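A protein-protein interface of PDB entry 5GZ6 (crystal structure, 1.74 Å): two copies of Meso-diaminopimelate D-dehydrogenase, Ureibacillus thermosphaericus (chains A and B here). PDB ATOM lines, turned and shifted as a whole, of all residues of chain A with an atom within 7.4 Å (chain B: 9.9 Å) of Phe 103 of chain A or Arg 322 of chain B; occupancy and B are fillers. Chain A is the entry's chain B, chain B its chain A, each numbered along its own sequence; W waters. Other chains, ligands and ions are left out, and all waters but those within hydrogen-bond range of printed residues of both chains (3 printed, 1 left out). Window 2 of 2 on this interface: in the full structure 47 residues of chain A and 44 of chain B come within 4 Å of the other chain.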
ATOM      1  N   PRO A  81     -36.816   0.224  36.562  1.00  0.00           N
ATOM      2  CA  PRO A  81     -36.175  -0.051  37.903  1.00  0.00           C
ATOM      3  C   PRO A  81     -37.269  -0.150  39.044  1.00  0.00           C
ATOM      4  O   PRO A  81     -37.067  -0.774  40.094  1.00  0.00           O
ATOM      5  CB  PRO A  81     -35.199   1.129  38.068  1.00  0.00           C
ATOM      6  CG  PRO A  81     -35.040   1.748  36.671  1.00  0.00           C
ATOM      7  CD  PRO A  81     -36.369   1.494  35.961  1.00  0.00           C
ATOM      8  N   PHE A  93     -36.556  -2.092  26.112  1.00  0.00           N
ATOM      9  CA  PHE A  93     -35.895  -0.795  26.161  1.00  0.00           C
ATOM     10  C   PHE A  93     -34.987  -0.684  24.953  1.00  0.00           C
ATOM     11  O   PHE A  93     -34.148  -1.546  24.709  1.00  0.00           O
ATOM     12  CB  PHE A  93     -35.095  -0.660  27.456  1.00  0.00           C
ATOM     13  CG  PHE A  93     -34.501   0.700  27.665  1.00  0.00           C
ATOM     14  CD1 PHE A  93     -35.302   1.774  28.017  1.00  0.00           C
ATOM     15  CD2 PHE A  93     -33.143   0.905  27.521  1.00  0.00           C
ATOM     16  CE1 PHE A  93     -34.759   3.025  28.214  1.00  0.00           C
ATOM     17  CE2 PHE A  93     -32.593   2.155  27.718  1.00  0.00           C
ATOM     18  CZ  PHE A  93     -33.402   3.218  28.065  1.00  0.00           C
ATOM     19  N   HIS A  96     -30.201   2.947  22.987  1.00  0.00           N
ATOM     20  CA  HIS A  96     -28.869   2.361  23.049  1.00  0.00           C
ATOM     21  C   HIS A  96     -27.880   3.153  23.881  1.00  0.00           C
ATOM     22  O   HIS A  96     -27.102   2.578  24.633  1.00  0.00           O
ATOM     23  CB  HIS A  96     -28.300   2.181  21.640  1.00  0.00           C
ATOM     24  CG  HIS A  96     -29.102   1.265  20.771  1.00  0.00           C
ATOM     25  ND1 HIS A  96     -29.021  -0.106  20.860  1.00  0.00           N
ATOM     26  CD2 HIS A  96     -29.987   1.525  19.781  1.00  0.00           C
ATOM     27  CE1 HIS A  96     -29.828  -0.652  19.970  1.00  0.00           C
ATOM     28  NE2 HIS A  96     -30.425   0.316  19.301  1.00  0.00           N
ATOM     29  N   ARG A  98     -28.458   4.955  26.397  1.00  0.00           N
ATOM     30  CA  ARG A  98     -28.834   4.882  27.792  1.00  0.00           C
ATOM     31  C   ARG A  98     -28.897   3.486  28.328  1.00  0.00           C
ATOM     32  O   ARG A  98     -29.277   3.288  29.476  1.00  0.00           O
ATOM     33  CB  ARG A  98     -30.266   5.487  27.933  1.00  0.00           C
ATOM     34  CG  ARG A  98     -30.334   6.942  27.425  1.00  0.00           C
ATOM     35  CD  ARG A  98     -29.673   7.858  28.441  1.00  0.00           C
ATOM     36  NE  ARG A  98     -30.343   7.622  29.740  1.00  0.00           N
ATOM     37  CZ  ARG A  98     -29.814   7.745  30.960  1.00  0.00           C
ATOM     38  NH1 ARG A  98     -28.558   8.127  31.143  1.00  0.00           N
ATOM     39  NH2 ARG A  98     -30.571   7.472  32.019  1.00  0.00           N
ATOM     40  N   ILE A  99     -28.665   2.473  27.482  1.00  0.00           N
ATOM     41  CA  ILE A  99     -28.720   1.099  27.975  1.00  0.00           C
ATOM     42  C   ILE A  99     -27.796   0.837  29.175  1.00  0.00           C
ATOM     43  O   ILE A  99     -28.178   0.202  30.153  1.00  0.00           O
ATOM     44  CB  ILE A  99     -28.549   0.103  26.818  1.00  0.00           C
ATOM     45  CG1 ILE A  99     -29.846  -0.094  26.117  1.00  0.00           C
ATOM     46  CG2 ILE A  99     -28.052  -1.245  27.323  1.00  0.00           C
ATOM     47  CD1 ILE A  99     -29.734  -0.781  24.783  1.00  0.00           C
ATOM     48  N   PRO A 100     -26.556   1.310  29.145  1.00  0.00           N
ATOM     49  CA  PRO A 100     -25.805   0.888  30.336  1.00  0.00           C
ATOM     50  C   PRO A 100     -26.355   1.439  31.672  1.00  0.00           C
ATOM     51  O   PRO A 100     -26.373   0.716  32.714  1.00  0.00           O
ATOM     52  CB  PRO A 100     -24.423   1.475  30.099  1.00  0.00           C
ATOM     53  CG  PRO A 100     -24.266   1.535  28.598  1.00  0.00           C
ATOM     54  CD  PRO A 100     -25.676   1.818  28.073  1.00  0.00           C
ATOM     55  N   ASP A 101     -26.791   2.690  31.641  1.00  0.00           N
ATOM     56  CA  ASP A 101     -27.365   3.338  32.805  1.00  0.00           C
ATOM     57  C   ASP A 101     -28.641   2.611  33.200  1.00  0.00           C
ATOM     58  O   ASP A 101     -28.906   2.404  34.380  1.00  0.00           O
ATOM     59  CB  ASP A 101     -27.716   4.792  32.485  1.00  0.00           C
ATOM     60  CG  ASP A 101     -26.536   5.730  32.619  1.00  0.00           C
ATOM     61  OD1 ASP A 101     -25.494   5.325  33.167  1.00  0.00           O
ATOM     62  OD2 ASP A 101     -26.657   6.883  32.172  1.00  0.00           O
ATOM     63  N   TYR A 102     -29.429   2.224  32.199  1.00  0.00           N
ATOM     64  CA  TYR A 102     -30.709   1.556  32.438  1.00  0.00           C
ATOM     65  C   TYR A 102     -30.500   0.155  33.026  1.00  0.00           C
ATOM     66  O   TYR A 102     -31.218  -0.262  33.951  1.00  0.00           O
ATOM     67  CB  TYR A 102     -31.619   1.446  31.179  1.00  0.00           C
ATOM     68  CG  TYR A 102     -32.970   0.713  31.328  1.00  0.00           C
ATOM     69  CD1 TYR A 102     -34.077   1.321  32.004  1.00  0.00           C
ATOM     70  CD2 TYR A 102     -33.186  -0.585  30.810  1.00  0.00           C
ATOM     71  CE1 TYR A 102     -35.316   0.702  32.059  1.00  0.00           C
ATOM     72  CE2 TYR A 102     -34.421  -1.206  30.910  1.00  0.00           C
ATOM     73  CZ  TYR A 102     -35.467  -0.571  31.611  1.00  0.00           C
ATOM     74  OH  TYR A 102     -36.674  -1.212  31.680  1.00  0.00           O
ATOM     75  N   PHE A 103     -29.572  -0.602  32.451  1.00  0.00           N
ATOM     76  CA  PHE A 103     -29.280  -1.928  32.929  1.00  0.00           C
ATOM     77  C   PHE A 103     -28.892  -1.869  34.440  1.00  0.00           C
ATOM     78  O   PHE A 103     -29.316  -2.727  35.249  1.00  0.00           O
ATOM     79  CB  PHE A 103     -28.033  -2.455  32.165  1.00  0.00           C
ATOM     80  CG  PHE A 103     -27.561  -3.739  32.678  1.00  0.00           C
ATOM     81  CD1 PHE A 103     -28.141  -4.940  32.238  1.00  0.00           C
ATOM     82  CD2 PHE A 103     -26.517  -3.774  33.655  1.00  0.00           C
ATOM     83  CE1 PHE A 103     -27.658  -6.142  32.777  1.00  0.00           C
ATOM     84  CE2 PHE A 103     -26.114  -4.956  34.204  1.00  0.00           C
ATOM     85  CZ  PHE A 103     -26.672  -6.147  33.799  1.00  0.00           C
ATOM     86  N   ASP A 104     -28.010  -0.923  34.745  1.00  0.00           N
ATOM     87  CA  ASP A 104     -27.471  -0.698  36.101  1.00  0.00           C
ATOM     88  C   ASP A 104     -28.637  -0.399  37.120  1.00  0.00           C
ATOM     89  O   ASP A 104     -28.712  -1.058  38.172  1.00  0.00           O
ATOM     90  CB  ASP A 104     -26.434   0.426  36.100  1.00  0.00           C
ATOM     91  CG  ASP A 104     -25.043  -0.003  35.553  1.00  0.00           C
ATOM     92  OD1 ASP A 104     -24.742  -1.209  35.366  1.00  0.00           O
ATOM     93  OD2 ASP A 104     -24.251   0.902  35.290  1.00  0.00           O
ATOM     94  N   ALA A 105     -29.544   0.516  36.757  1.00  0.00           N
ATOM     95  CA  ALA A 105     -30.632   0.907  37.616  1.00  0.00           C
ATOM     96  C   ALA A 105     -31.544  -0.286  37.826  1.00  0.00           C
ATOM     97  O   ALA A 105     -31.933  -0.611  38.978  1.00  0.00           O
ATOM     98  CB  ALA A 105     -31.426   2.073  37.043  1.00  0.00           C
ATOM     99  N   VAL A 106     -31.848  -0.988  36.736  1.00  0.00           N
ATOM    100  CA  VAL A 106     -32.630  -2.195  36.793  1.00  0.00           C
ATOM    101  C   VAL A 106     -31.959  -3.322  37.560  1.00  0.00           C
ATOM    102  O   VAL A 106     -32.610  -3.991  38.386  1.00  0.00           O
ATOM    103  CB  VAL A 106     -33.067  -2.728  35.387  1.00  0.00           C
ATOM    104  CG1 VAL A 106     -33.820  -3.988  35.523  1.00  0.00           C
ATOM    105  CG2 VAL A 106     -33.882  -1.754  34.593  1.00  0.00           C
ATOM    106  N   ASN A 107     -30.673  -3.520  37.354  1.00  0.00           N
ATOM    107  CA  ASN A 107     -29.925  -4.527  38.050  1.00  0.00           C
ATOM    108  C   ASN A 107     -29.891  -4.238  39.585  1.00  0.00           C
ATOM    109  O   ASN A 107     -29.972  -5.148  40.326  1.00  0.00           O
ATOM    110  CB  ASN A 107     -28.496  -4.585  37.539  1.00  0.00           C
ATOM    111  CG  ASN A 107     -27.756  -5.793  38.009  1.00  0.00           C
ATOM    112  OD1 ASN A 107     -28.258  -6.908  38.034  1.00  0.00           O
ATOM    113  ND2 ASN A 107     -26.537  -5.555  38.453  1.00  0.00           N
ATOM    114  N   ALA A 108     -29.708  -2.982  39.969  1.00  0.00           N
ATOM    115  CA  ALA A 108     -29.640  -2.614  41.407  1.00  0.00           C
ATOM    116  C   ALA A 108     -31.010  -2.951  42.033  1.00  0.00           C
ATOM    117  O   ALA A 108     -31.101  -3.655  43.052  1.00  0.00           O
ATOM    118  CB  ALA A 108     -29.312  -1.150  41.545  1.00  0.00           C
ATOM    119  N   ALA A 109     -32.092  -2.527  41.385  1.00  0.00           N
ATOM    120  CA  ALA A 109     -33.410  -2.995  41.865  1.00  0.00           C
ATOM    121  C   ALA A 109     -33.531  -4.514  41.931  1.00  0.00           C
ATOM    122  O   ALA A 109     -33.877  -5.076  42.988  1.00  0.00           O
ATOM    123  CB  ALA A 109     -34.541  -2.402  41.122  1.00  0.00           C
ATOM    124  N   ALA A 110     -33.237  -5.187  40.845  1.00  0.00           N
ATOM    125  CA  ALA A 110     -33.504  -6.617  40.695  1.00  0.00           C
ATOM    126  C   ALA A 110     -32.602  -7.490  41.597  1.00  0.00           C
ATOM    127  O   ALA A 110     -33.039  -8.555  42.078  1.00  0.00           O
ATOM    128  CB  ALA A 110     -33.324  -7.049  39.233  1.00  0.00           C
ATOM    129  N   ALA A 117     -34.674  -9.718  35.710  1.00  0.00           N
ATOM    130  CA  ALA A 117     -35.231  -8.797  34.761  1.00  0.00           C
ATOM    131  C   ALA A 117     -34.485  -8.890  33.429  1.00  0.00           C
ATOM    132  O   ALA A 117     -33.260  -8.946  33.402  1.00  0.00           O
ATOM    133  CB  ALA A 117     -35.128  -7.408  35.219  1.00  0.00           C
ATOM    134  N   ILE A 119     -33.848  -7.106  29.980  1.00  0.00           N
ATOM    135  CA  ILE A 119     -34.009  -5.818  29.359  1.00  0.00           C
ATOM    136  C   ILE A 119     -33.807  -5.965  27.864  1.00  0.00           C
ATOM    137  O   ILE A 119     -33.069  -6.869  27.463  1.00  0.00           O
ATOM    138  CB  ILE A 119     -33.086  -4.778  29.960  1.00  0.00           C
ATOM    139  CG1 ILE A 119     -31.567  -5.000  29.719  1.00  0.00           C
ATOM    140  CG2 ILE A 119     -33.353  -4.641  31.484  1.00  0.00           C
ATOM    141  CD1 ILE A 119     -30.876  -3.668  29.643  1.00  0.00           C
ATOM    142  N   SER A 120     -34.395  -5.028  27.114  1.00  0.00           N
ATOM    143  CA  SER A 120     -33.953  -4.750  25.742  1.00  0.00           C
ATOM    144  C   SER A 120     -34.095  -5.992  24.845  1.00  0.00           C
ATOM    145  O   SER A 120     -33.212  -6.287  24.008  1.00  0.00           O
ATOM    146  CB  SER A 120     -32.521  -4.251  25.797  1.00  0.00           C
ATOM    147  OG  SER A 120     -32.381  -3.048  26.464  1.00  0.00           O
ATOM    148  N   GLY A 301     -31.272 -10.522  39.253  1.00  0.00           N
ATOM    149  CA  GLY A 301     -30.630  -9.376  38.648  1.00  0.00           C
ATOM    150  C   GLY A 301     -30.943  -9.218  37.175  1.00  0.00           C
ATOM    151  O   GLY A 301     -31.610 -10.054  36.576  1.00  0.00           O
ATOM    152  N   ALA A 302     -30.459  -8.124  36.601  1.00  0.00           N
ATOM    153  CA  ALA A 302     -30.678  -7.822  35.196  1.00  0.00           C
ATOM    154  C   ALA A 302     -29.898  -8.730  34.249  1.00  0.00           C
ATOM    155  O   ALA A 302     -28.756  -9.090  34.507  1.00  0.00           O
ATOM    156  CB  ALA A 302     -30.358  -6.362  34.916  1.00  0.00           C
ATOM    157  N   LYS A 303     -30.549  -9.075  33.148  1.00  0.00           N
ATOM    158  CA  LYS A 303     -30.002  -9.920  32.071  1.00  0.00           C
ATOM    159  C   LYS A 303     -30.290  -9.228  30.703  1.00  0.00           C
ATOM    160  O   LYS A 303     -31.250  -8.438  30.524  1.00  0.00           O
ATOM    161  CB  LYS A 303     -30.709 -11.230  31.989  1.00  0.00           C
ATOM    162  CG  LYS A 303     -30.862 -11.992  33.310  1.00  0.00           C
ATOM    163  CD  LYS A 303     -29.504 -12.364  33.922  1.00  0.00           C
ATOM    164  CE  LYS A 303     -29.690 -12.946  35.320  1.00  0.00           C
ATOM    165  NZ  LYS A 303     -28.399 -13.413  35.798  1.00  0.00           N
ATOM    166  N   THR A 304     -29.488  -9.496  29.664  1.00  0.00           N
ATOM    167  CA  THR A 304     -29.845  -9.005  28.333  1.00  0.00           C
ATOM    168  C   THR A 304     -29.815 -10.257  27.470  1.00  0.00           C
ATOM    169  O   THR A 304     -29.483 -11.353  27.929  1.00  0.00           O
ATOM    170  CB  THR A 304     -28.762  -8.031  27.794  1.00  0.00           C
ATOM    171  OG1 THR A 304     -27.565  -8.782  27.479  1.00  0.00           O
ATOM    172  CG2 THR A 304     -28.471  -7.083  28.855  1.00  0.00           C
ATOM    173  N   PHE A 306     -27.650 -11.190  25.580  1.00  0.00           N
ATOM    174  CA  PHE A 306     -26.356 -11.790  25.559  1.00  0.00           C
ATOM    175  C   PHE A 306     -26.188 -12.888  26.680  1.00  0.00           C
ATOM    176  O   PHE A 306     -25.270 -13.635  26.682  1.00  0.00           O
ATOM    177  CB  PHE A 306     -25.291 -10.766  25.784  1.00  0.00           C
ATOM    178  CG  PHE A 306     -25.167  -9.763  24.652  1.00  0.00           C
ATOM    179  CD1 PHE A 306     -25.520 -10.120  23.373  1.00  0.00           C
ATOM    180  CD2 PHE A 306     -24.747  -8.488  24.848  1.00  0.00           C
ATOM    181  CE1 PHE A 306     -25.417  -9.239  22.267  1.00  0.00           C
ATOM    182  CE2 PHE A 306     -24.631  -7.599  23.789  1.00  0.00           C
ATOM    183  CZ  PHE A 306     -25.026  -7.946  22.513  1.00  0.00           C
ATOM    184  N   ASP A 307     -27.104 -12.921  27.630  1.00  0.00           N
ATOM    185  CA  ASP A 307     -27.003 -13.777  28.837  1.00  0.00           C
ATOM    186  C   ASP A 307     -27.940 -14.945  28.758  1.00  0.00           C
ATOM    187  O   ASP A 307     -27.869 -15.844  29.623  1.00  0.00           O
ATOM    188  CB  ASP A 307     -27.422 -12.941  30.081  1.00  0.00           C
ATOM    189  CG  ASP A 307     -26.537 -11.779  30.329  1.00  0.00           C
ATOM    190  OD1 ASP A 307     -25.304 -11.919  30.184  1.00  0.00           O
ATOM    191  OD2 ASP A 307     -27.020 -10.660  30.592  1.00  0.00           O
ATOM    192  N   GLY B 311     -22.779 -13.910  25.086  1.00  0.00           N
ATOM    193  CA  GLY B 311     -21.713 -13.142  25.695  1.00  0.00           C
ATOM    194  C   GLY B 311     -20.444 -13.959  25.848  1.00  0.00           C
ATOM    195  O   GLY B 311     -19.345 -13.430  25.739  1.00  0.00           O
ATOM    196  N   SER B 314     -17.470 -13.926  23.115  1.00  0.00           N
ATOM    197  CA  SER B 314     -16.663 -12.751  22.979  1.00  0.00           C
ATOM    198  C   SER B 314     -15.665 -12.582  24.107  1.00  0.00           C
ATOM    199  O   SER B 314     -15.973 -12.817  25.293  1.00  0.00           O
ATOM    200  CB  SER B 314     -17.519 -11.466  22.974  1.00  0.00           C
ATOM    201  OG  SER B 314     -16.695 -10.305  23.035  1.00  0.00           O
ATOM    202  N   LYS B 316     -14.652  -9.720  25.041  1.00  0.00           N
ATOM    203  CA  LYS B 316     -15.029  -8.485  25.724  1.00  0.00           C
ATOM    204  C   LYS B 316     -15.820  -8.761  27.027  1.00  0.00           C
ATOM    205  O   LYS B 316     -16.456  -9.820  27.242  1.00  0.00           O
ATOM    206  CB  LYS B 316     -15.796  -7.566  24.822  1.00  0.00           C
ATOM    207  CG  LYS B 316     -15.088  -7.232  23.556  1.00  0.00           C
ATOM    208  CD  LYS B 316     -15.894  -6.299  22.665  1.00  0.00           C
ATOM    209  CE  LYS B 316     -15.100  -5.997  21.426  1.00  0.00           C
ATOM    210  NZ  LYS B 316     -15.738  -5.156  20.430  1.00  0.00           N
ATOM    211  N   SER B 317     -15.746  -7.813  27.929  1.00  0.00           N
ATOM    212  CA  SER B 317     -16.475  -7.937  29.167  1.00  0.00           C
ATOM    213  C   SER B 317     -18.021  -7.752  28.931  1.00  0.00           C
ATOM    214  O   SER B 317     -18.417  -7.177  27.969  1.00  0.00           O
ATOM    215  CB  SER B 317     -16.040  -6.869  30.152  1.00  0.00           C
ATOM    216  OG  SER B 317     -16.537  -5.571  29.809  1.00  0.00           O
ATOM    217  N   PRO B 318     -18.862  -8.334  29.791  1.00  0.00           N
ATOM    218  CA  PRO B 318     -20.306  -8.166  29.611  1.00  0.00           C
ATOM    219  C   PRO B 318     -20.695  -6.712  29.553  1.00  0.00           C
ATOM    220  O   PRO B 318     -21.527  -6.303  28.721  1.00  0.00           O
ATOM    221  CB  PRO B 318     -20.900  -8.881  30.828  1.00  0.00           C
ATOM    222  CG  PRO B 318     -19.845  -9.945  31.190  1.00  0.00           C
ATOM    223  CD  PRO B 318     -18.535  -9.334  30.843  1.00  0.00           C
ATOM    224  N   GLU B 319     -20.076  -5.857  30.384  1.00  0.00           N
ATOM    225  CA  GLU B 319     -20.424  -4.481  30.378  1.00  0.00           C
ATOM    226  C   GLU B 319     -19.998  -3.799  29.103  1.00  0.00           C
ATOM    227  O   GLU B 319     -20.772  -2.982  28.513  1.00  0.00           O
ATOM    228  CB  GLU B 319     -19.834  -3.792  31.655  1.00  0.00           C
ATOM    229  CG  GLU B 319     -19.978  -2.291  31.587  1.00  0.00           C
ATOM    230  CD  GLU B 319     -19.621  -1.535  32.882  1.00  0.00           C
ATOM    231  OE1 GLU B 319     -18.573  -1.801  33.483  1.00  0.00           O
ATOM    232  OE2 GLU B 319     -20.386  -0.591  33.223  1.00  0.00           O
ATOM    233  N   ASP B 320     -18.817  -4.154  28.553  1.00  0.00           N
ATOM    234  CA  ASP B 320     -18.474  -3.643  27.242  1.00  0.00           C
ATOM    235  C   ASP B 320     -19.410  -4.115  26.108  1.00  0.00           C
ATOM    236  O   ASP B 320     -19.716  -3.259  25.242  1.00  0.00           O
ATOM    237  CB  ASP B 320     -17.029  -3.847  26.840  1.00  0.00           C
ATOM    238  CG  ASP B 320     -16.038  -2.964  27.689  1.00  0.00           C
ATOM    239  OD1 ASP B 320     -16.391  -1.881  28.198  1.00  0.00           O
ATOM    240  OD2 ASP B 320     -14.897  -3.379  27.735  1.00  0.00           O
ATOM    241  N   LEU B 321     -19.888  -5.350  26.138  1.00  0.00           N
ATOM    242  CA  LEU B 321     -20.772  -5.793  25.092  1.00  0.00           C
ATOM    243  C   LEU B 321     -22.077  -5.022  25.189  1.00  0.00           C
ATOM    244  O   LEU B 321     -22.672  -4.626  24.170  1.00  0.00           O
ATOM    245  CB  LEU B 321     -21.094  -7.276  25.285  1.00  0.00           C
ATOM    246  CG  LEU B 321     -19.877  -8.162  25.019  1.00  0.00           C
ATOM    247  CD1 LEU B 321     -20.277  -9.572  25.494  1.00  0.00           C
ATOM    248  CD2 LEU B 321     -19.498  -8.112  23.539  1.00  0.00           C
ATOM    249  N   ARG B 322     -22.613  -4.826  26.405  1.00  0.00           N
ATOM    250  CA  ARG B 322     -23.806  -3.946  26.540  1.00  0.00           C
ATOM    251  C   ARG B 322     -23.638  -2.557  26.053  1.00  0.00           C
ATOM    252  O   ARG B 322     -24.428  -2.040  25.275  1.00  0.00           O
ATOM    253  CB  ARG B 322     -24.344  -3.911  27.957  1.00  0.00           C
ATOM    254  CG  ARG B 322     -24.780  -5.217  28.459  1.00  0.00           C
ATOM    255  CD  ARG B 322     -25.519  -5.089  29.787  1.00  0.00           C
ATOM    256  NE  ARG B 322     -24.602  -4.714  30.907  1.00  0.00           N
ATOM    257  CZ  ARG B 322     -23.921  -5.595  31.661  1.00  0.00           C
ATOM    258  NH1 ARG B 322     -23.992  -6.884  31.491  1.00  0.00           N
ATOM    259  NH2 ARG B 322     -23.075  -5.175  32.604  1.00  0.00           N
ATOM    260  N   LYS B 323     -22.507  -1.957  26.363  1.00  0.00           N
ATOM    261  CA  LYS B 323     -22.232  -0.630  25.883  1.00  0.00           C
ATOM    262  C   LYS B 323     -22.071  -0.472  24.333  1.00  0.00           C
ATOM    263  O   LYS B 323     -22.610   0.468  23.726  1.00  0.00           O
ATOM    264  CB  LYS B 323     -20.927  -0.207  26.598  1.00  0.00           C
ATOM    265  CG  LYS B 323     -20.443   1.189  26.448  1.00  0.00           C
ATOM    266  CD  LYS B 323     -19.480   1.542  27.622  1.00  0.00           C
ATOM    267  CE  LYS B 323     -18.378   2.487  27.140  1.00  0.00           C
ATOM    268  NZ  LYS B 323     -18.947   3.676  26.443  1.00  0.00           N
ATOM    269  N   GLU B 324     -21.363  -1.419  23.708  1.00  0.00           N
ATOM    270  CA  GLU B 324     -20.926  -1.278  22.377  1.00  0.00           C
ATOM    271  C   GLU B 324     -21.932  -1.869  21.362  1.00  0.00           C
ATOM    272  O   GLU B 324     -22.149  -1.296  20.298  1.00  0.00           O
ATOM    273  CB  GLU B 324     -19.573  -1.956  22.191  1.00  0.00           C
ATOM    274  CG  GLU B 324     -18.381  -1.280  22.830  1.00  0.00           C
ATOM    275  CD  GLU B 324     -17.128  -2.224  22.820  1.00  0.00           C
ATOM    276  OE1 GLU B 324     -16.996  -3.064  21.860  1.00  0.00           O
ATOM    277  OE2 GLU B 324     -16.306  -2.051  23.723  1.00  0.00           O
ATOM    278  N   LEU B 325     -22.591  -2.958  21.753  1.00  0.00           N
ATOM    279  CA  LEU B 325     -23.385  -3.784  20.811  1.00  0.00           C
ATOM    280  C   LEU B 325     -24.867  -3.875  21.056  1.00  0.00           C
ATOM    281  O   LEU B 325     -25.610  -4.132  20.144  1.00  0.00           O
ATOM    282  CB  LEU B 325     -22.870  -5.223  20.737  1.00  0.00           C
ATOM    283  CG  LEU B 325     -21.402  -5.463  20.469  1.00  0.00           C
ATOM    284  CD1 LEU B 325     -21.163  -6.902  20.206  1.00  0.00           C
ATOM    285  CD2 LEU B 325     -20.856  -4.618  19.351  1.00  0.00           C
ATOM    286  N   LEU B 326     -25.315  -3.632  22.252  1.00  0.00           N
ATOM    287  CA  LEU B 326     -26.744  -4.021  22.549  1.00  0.00           C
ATOM    288  C   LEU B 326     -27.642  -3.028  21.924  1.00  0.00           C
ATOM    289  O   LEU B 326     -27.408  -1.825  22.161  1.00  0.00           O
ATOM    290  CB  LEU B 326     -26.935  -4.183  24.041  1.00  0.00           C
ATOM    291  CG  LEU B 326     -28.245  -4.727  24.436  1.00  0.00           C
ATOM    292  CD1 LEU B 326     -28.361  -6.200  24.050  1.00  0.00           C
ATOM    293  CD2 LEU B 326     -28.433  -4.769  26.001  1.00  0.00           C
ATOM    294  OXT LEU B 326     -28.564  -3.394  21.107  1.00  0.00           O
HETATM  295  O   HOH W   1     -25.652  -8.571  29.453  1.00  0.00           O
HETATM  296  O   HOH W   2     -24.435   2.102  24.925  1.00  0.00           O
HETATM  297  O   HOH W   3     -23.044 -14.646  28.459  1.00  0.00           O
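ND1 of His 96 of chain A lies within hydrogen-bond range of O of Leu 326 of chain B, 2.7 Å away.
The backbone NH of Gly 311 of chain B lies within hydrogen-bond range of the backbone carbonyl oxygen of Phe 306 of chain A, 3.0 Å away.
Hydrophobic or aromatic side chains of chain B within 4 Å of the printed part of chain A: Leu 321, Leu 325 and Leu 326.
Hydrophobic or aromatic side chains of chain A within 4 Å of the printed part of chain B: His 96, Ile 99, Phe 103 and Phe 306.
Water W2 bridges O of His 96 of chain A (2.7 Å) and O of Lys 323 of chain B (2.7 Å).
Water W1 lies within hydrogen-bond range of OD2 of Asp 307 of chain A (2.7 Å), OG1 of Thr 304 of chain A (2.8 Å) and NH1 of Arg 322 of chain B (3.1 Å).
Water W3 lies within hydrogen-bond range of the backbone carbonyl oxygen (O) of Phe 306 of chain A (3.0 Å) and the backbone NH (N) of Gly 311 of chain B (3.5 Å).
No position is printed for both chains.
Ile 99 of chain A touches Leu 326 of chain B (CD1 to O, 3.7 Å).
Phe 103 of chain A touches Arg 322 of chain B.
CG2 of Thr 304 of chain A touches CD of Arg 322 of chain B, 3.7 Å away.
CD2 of Leu 326 of chain B touches CG2 of Thr 304 of chain A, 3.7 Å away.
Phe 306 of chain A touches Leu 321 of chain B.
CB of Leu 325 of chain B touches CZ of Phe 306 of chain A, at 3.9 Å.
CE2 of Phe 306 of chain A touches CD1 of Leu 326 of chain B, at 3.99 Å.
The side-chain hydroxyl (OG1) of Thr 304 of chain A sits close to the backbone NH (N) of Phe 306 of chain A (3.1 Å).
The backbone carbonyl oxygen (O) of Leu 321 of chain B is in hydrogen-bond range of the backbone NH (N) of Leu 326 of chain B.
N of Thr 304 of chain A lies within hydrogen-bond range of OD2 of Asp 307 of chain A, 2.9 Å away.
Of chain B, only Arg 322 comes within 4 Å of Phe 103 of chain A.
Of chain A, only Phe 103 (3.4 Å) and Thr 304 (3.7 Å) come within 4 Å of Arg 322 of chain B.
No residue of chain B comes within 4 Å of Pro 100 of chain A.
No residue of chain B comes within 4 Å of Asp 104 of chain A.
No residue of chain B comes within 4 Å of Ala 105 of chain A.
Val 106 of chain A touches none of the printed residues of chain B.
Asn 107 of chain A touches none of the printed residues of chain B.
No residue of chain B comes within 4 Å of Ala 302 of chain A.
Printed residues of chain B within 4 Å of Ile 99 of chain A: Leu 326.
Printed residues of chain A within 4 Å of Leu 321 of chain B: Phe 306 (3.6 Å).
Ser 120 of chain A touches none of the printed residues of chain B.
The nearest residue of chain A that does not touch Arg 322 of chain B is Ile 99 of chain A (4.2 Å).
The nearest printed residue of chain B that does not touch His 96 of chain A is Lys 323 of chain B (5.0 Å).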
